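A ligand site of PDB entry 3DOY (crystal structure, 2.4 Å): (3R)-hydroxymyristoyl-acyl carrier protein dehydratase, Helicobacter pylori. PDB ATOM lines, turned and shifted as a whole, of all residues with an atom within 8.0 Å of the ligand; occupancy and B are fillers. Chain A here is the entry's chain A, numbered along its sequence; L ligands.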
ATOM      1  N   GLN A  37       7.737   1.561 -28.625  1.00  0.00           N
ATOM      2  CA  GLN A  37       6.329   1.510 -28.263  1.00  0.00           C
ATOM      3  C   GLN A  37       5.980   2.593 -27.247  1.00  0.00           C
ATOM      4  O   GLN A  37       6.429   2.543 -26.107  1.00  0.00           O
ATOM      5  CB  GLN A  37       5.987   0.141 -27.685  1.00  0.00           C
ATOM      6  CG  GLN A  37       4.520  -0.202 -27.746  1.00  0.00           C
ATOM      7  CD  GLN A  37       4.025  -0.327 -29.173  1.00  0.00           C
ATOM      8  OE1 GLN A  37       2.905   0.035 -29.479  1.00  0.00           O
ATOM      9  NE2 GLN A  37       4.867  -0.857 -30.037  1.00  0.00           N
ATOM     10  N   ALA A  38       5.189   3.561 -27.671  1.00  0.00           N
ATOM     11  CA  ALA A  38       4.802   4.681 -26.836  1.00  0.00           C
ATOM     12  C   ALA A  38       4.368   4.301 -25.418  1.00  0.00           C
ATOM     13  O   ALA A  38       3.536   3.432 -25.237  1.00  0.00           O
ATOM     14  CB  ALA A  38       3.733   5.486 -27.510  1.00  0.00           C
ATOM     15  N   ASN A  39       4.943   4.973 -24.433  1.00  0.00           N
ATOM     16  CA  ASN A  39       4.598   4.789 -23.038  1.00  0.00           C
ATOM     17  C   ASN A  39       4.892   3.398 -22.506  1.00  0.00           C
ATOM     18  O   ASN A  39       4.521   3.048 -21.390  1.00  0.00           O
ATOM     19  CB  ASN A  39       3.147   5.186 -22.757  1.00  0.00           C
ATOM     20  CG  ASN A  39       2.801   6.544 -23.289  1.00  0.00           C
ATOM     21  OD1 ASN A  39       1.999   6.677 -24.211  1.00  0.00           O
ATOM     22  ND2 ASN A  39       3.412   7.573 -22.734  1.00  0.00           N
ATOM     23  N   GLN A  40       5.558   2.595 -23.318  1.00  0.00           N
ATOM     24  CA  GLN A  40       5.784   1.202 -22.995  1.00  0.00           C
ATOM     25  C   GLN A  40       7.243   0.793 -23.042  1.00  0.00           C
ATOM     26  O   GLN A  40       7.814   0.436 -22.039  1.00  0.00           O
ATOM     27  CB  GLN A  40       4.921   0.280 -23.846  1.00  0.00           C
ATOM     28  CG  GLN A  40       3.562   0.012 -23.249  1.00  0.00           C
ATOM     29  CD  GLN A  40       2.759  -0.983 -24.034  1.00  0.00           C
ATOM     30  OE1 GLN A  40       1.993  -0.613 -24.912  1.00  0.00           O
ATOM     31  NE2 GLN A  40       2.909  -2.242 -23.706  1.00  0.00           N
ATOM     32  N   LYS A  41       7.852   0.843 -24.226  1.00  0.00           N
ATOM     33  CA  LYS A  41       9.234   0.430 -24.287  1.00  0.00           C
ATOM     34  C   LYS A  41       9.997   0.845 -25.529  1.00  0.00           C
ATOM     35  O   LYS A  41       9.427   1.328 -26.509  1.00  0.00           O
ATOM     36  CB  LYS A  41       9.323  -1.084 -24.147  1.00  0.00           C
ATOM     37  CG  LYS A  41       8.802  -1.840 -25.355  1.00  0.00           C
ATOM     38  CD  LYS A  41       9.506  -3.188 -25.427  1.00  0.00           C
ATOM     39  CE  LYS A  41       9.034  -4.013 -26.604  1.00  0.00           C
ATOM     40  NZ  LYS A  41       9.836  -5.290 -26.679  1.00  0.00           N
ATOM     41  N   ILE A  42      11.306   0.642 -25.454  1.00  0.00           N
ATOM     42  CA  ILE A  42      12.191   0.947 -26.557  1.00  0.00           C
ATOM     43  C   ILE A  42      13.346  -0.048 -26.581  1.00  0.00           C
ATOM     44  O   ILE A  42      13.782  -0.557 -25.553  1.00  0.00           O
ATOM     45  CB  ILE A  42      12.738   2.391 -26.450  1.00  0.00           C
ATOM     46  CG1 ILE A  42      13.626   2.707 -27.656  1.00  0.00           C
ATOM     47  CG2 ILE A  42      13.507   2.580 -25.166  1.00  0.00           C
ATOM     48  CD1 ILE A  42      14.014   4.159 -27.778  1.00  0.00           C
ATOM     49  N   LEU A 123      14.789  -0.876 -22.676  1.00  0.00           N
ATOM     50  CA  LEU A 123      14.165  -0.093 -21.625  1.00  0.00           C
ATOM     51  C   LEU A 123      12.644  -0.210 -21.675  1.00  0.00           C
ATOM     52  O   LEU A 123      12.043  -0.225 -22.752  1.00  0.00           O
ATOM     53  CB  LEU A 123      14.561   1.389 -21.727  1.00  0.00           C
ATOM     54  CG  LEU A 123      15.957   1.803 -21.254  1.00  0.00           C
ATOM     55  CD1 LEU A 123      16.108   1.508 -19.766  1.00  0.00           C
ATOM     56  CD2 LEU A 123      17.019   1.056 -22.059  1.00  0.00           C
ATOM     57  N   GLU A 124      12.036  -0.263 -20.500  1.00  0.00           N
ATOM     58  CA  GLU A 124      10.595  -0.362 -20.391  1.00  0.00           C
ATOM     59  C   GLU A 124      10.089   0.686 -19.391  1.00  0.00           C
ATOM     60  O   GLU A 124      10.738   0.969 -18.380  1.00  0.00           O
ATOM     61  CB  GLU A 124      10.218  -1.785 -19.955  1.00  0.00           C
ATOM     62  CG  GLU A 124      11.038  -2.837 -20.710  1.00  0.00           C
ATOM     63  CD  GLU A 124      10.226  -3.973 -21.263  1.00  0.00           C
ATOM     64  OE1 GLU A 124      10.179  -5.044 -20.610  1.00  0.00           O
ATOM     65  OE2 GLU A 124       9.633  -3.802 -22.352  1.00  0.00           O
ATOM     66  N   VAL A 125       8.929   1.274 -19.685  1.00  0.00           N
ATOM     67  CA  VAL A 125       8.340   2.294 -18.829  1.00  0.00           C
ATOM     68  C   VAL A 125       7.689   1.682 -17.585  1.00  0.00           C
ATOM     69  O   VAL A 125       6.700   0.952 -17.688  1.00  0.00           O
ATOM     70  CB  VAL A 125       7.272   3.098 -19.600  1.00  0.00           C
ATOM     71  CG1 VAL A 125       6.663   4.172 -18.713  1.00  0.00           C
ATOM     72  CG2 VAL A 125       7.900   3.692 -20.837  1.00  0.00           C
ATOM     73  N   LEU A 126       8.234   1.988 -16.416  1.00  0.00           N
ATOM     74  CA  LEU A 126       7.703   1.457 -15.167  1.00  0.00           C
ATOM     75  C   LEU A 126       6.632   2.386 -14.591  1.00  0.00           C
ATOM     76  O   LEU A 126       5.713   1.946 -13.899  1.00  0.00           O
ATOM     77  CB  LEU A 126       8.839   1.236 -14.160  1.00  0.00           C
ATOM     78  CG  LEU A 126       9.863   0.193 -14.615  1.00  0.00           C
ATOM     79  CD1 LEU A 126      11.164   0.361 -13.849  1.00  0.00           C
ATOM     80  CD2 LEU A 126       9.301  -1.207 -14.415  1.00  0.00           C
ATOM     81  N   LYS A 127       6.753   3.683 -14.900  1.00  0.00           N
ATOM     82  CA  LYS A 127       5.775   4.669 -14.440  1.00  0.00           C
ATOM     83  C   LYS A 127       6.014   6.037 -15.066  1.00  0.00           C
ATOM     84  O   LYS A 127       7.126   6.574 -15.007  1.00  0.00           O
ATOM     85  CB  LYS A 127       5.826   4.790 -12.904  1.00  0.00           C
ATOM     86  CG  LYS A 127       4.992   5.939 -12.309  1.00  0.00           C
ATOM     87  CD  LYS A 127       5.098   5.938 -10.773  1.00  0.00           C
ATOM     88  CE  LYS A 127       4.306   7.070 -10.115  1.00  0.00           C
ATOM     89  NZ  LYS A 127       4.977   8.410 -10.317  1.00  0.00           N
ATOM     90  N   GLN A 134       9.951   6.980 -15.034  1.00  0.00           N
ATOM     91  CA  GLN A 134      10.761   5.976 -14.355  1.00  0.00           C
ATOM     92  C   GLN A 134      10.844   4.782 -15.283  1.00  0.00           C
ATOM     93  O   GLN A 134       9.831   4.195 -15.642  1.00  0.00           O
ATOM     94  CB  GLN A 134      10.111   5.562 -13.021  1.00  0.00           C
ATOM     95  CG  GLN A 134      10.056   6.692 -11.977  1.00  0.00           C
ATOM     96  CD  GLN A 134       9.026   6.460 -10.868  1.00  0.00           C
ATOM     97  OE1 GLN A 134       9.092   5.450 -10.149  1.00  0.00           O
ATOM     98  NE2 GLN A 134       8.069   7.395 -10.712  1.00  0.00           N
ATOM     99  N   GLY A 136      13.198   1.103 -16.520  1.00  0.00           N
ATOM    100  CA  GLY A 136      14.088   0.071 -16.054  1.00  0.00           C
ATOM    101  C   GLY A 136      14.323  -0.874 -17.198  1.00  0.00           C
ATOM    102  O   GLY A 136      13.471  -0.987 -18.095  1.00  0.00           O
HETATM  103  C1  LIG L   1       6.455  -3.045 -20.150  1.00  0.00           C
HETATM  104  C2  LIG L   1       6.116  -2.046 -19.240  1.00  0.00           C
HETATM  105  C3  LIG L   1       6.539  -2.134 -17.922  1.00  0.00           C
HETATM  106  C4  LIG L   1       7.301  -3.218 -17.505  1.00  0.00           C
HETATM  107  C5  LIG L   1       7.640  -4.214 -18.406  1.00  0.00           C
HETATM  108  C6  LIG L   1       7.217  -4.129 -19.733  1.00  0.00           C
HETATM  109  C7  LIG L   1       5.985  -2.992 -21.455  1.00  0.00           C
HETATM  110  N1  LIG L   1       4.889  -2.303 -21.745  1.00  0.00           N
HETATM  111  N2  LIG L   1       6.651  -3.617 -22.429  1.00  0.00           N
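Val 125 touches the ligand.
Within 4 Å of the ligand: Gln 40, Glu 124 and Val 125.
Along chain A the residues within 4 Å of the ligand span positions 40 to 125.
The nearest printed residue that does not touch the ligand is Lys 41 (4.04 Å).
NE2 of Gln 40 sits close to N1 of the ligand (2.8 Å).
The side-chain carboxylate (OE2) of Glu 124 is in salt-bridge range of a nitrogen (N2) of the ligand (3.0 Å).
The backbone carbonyl oxygen of Gln 40 is in hydrogen-bond range of the backbone NH of Val 125 (2.7 Å).
The backbone carbonyl oxygen (O) of Gly 136 lies within hydrogen-bond range of the backbone NH (N) of Glu 124, at 2.9 Å.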
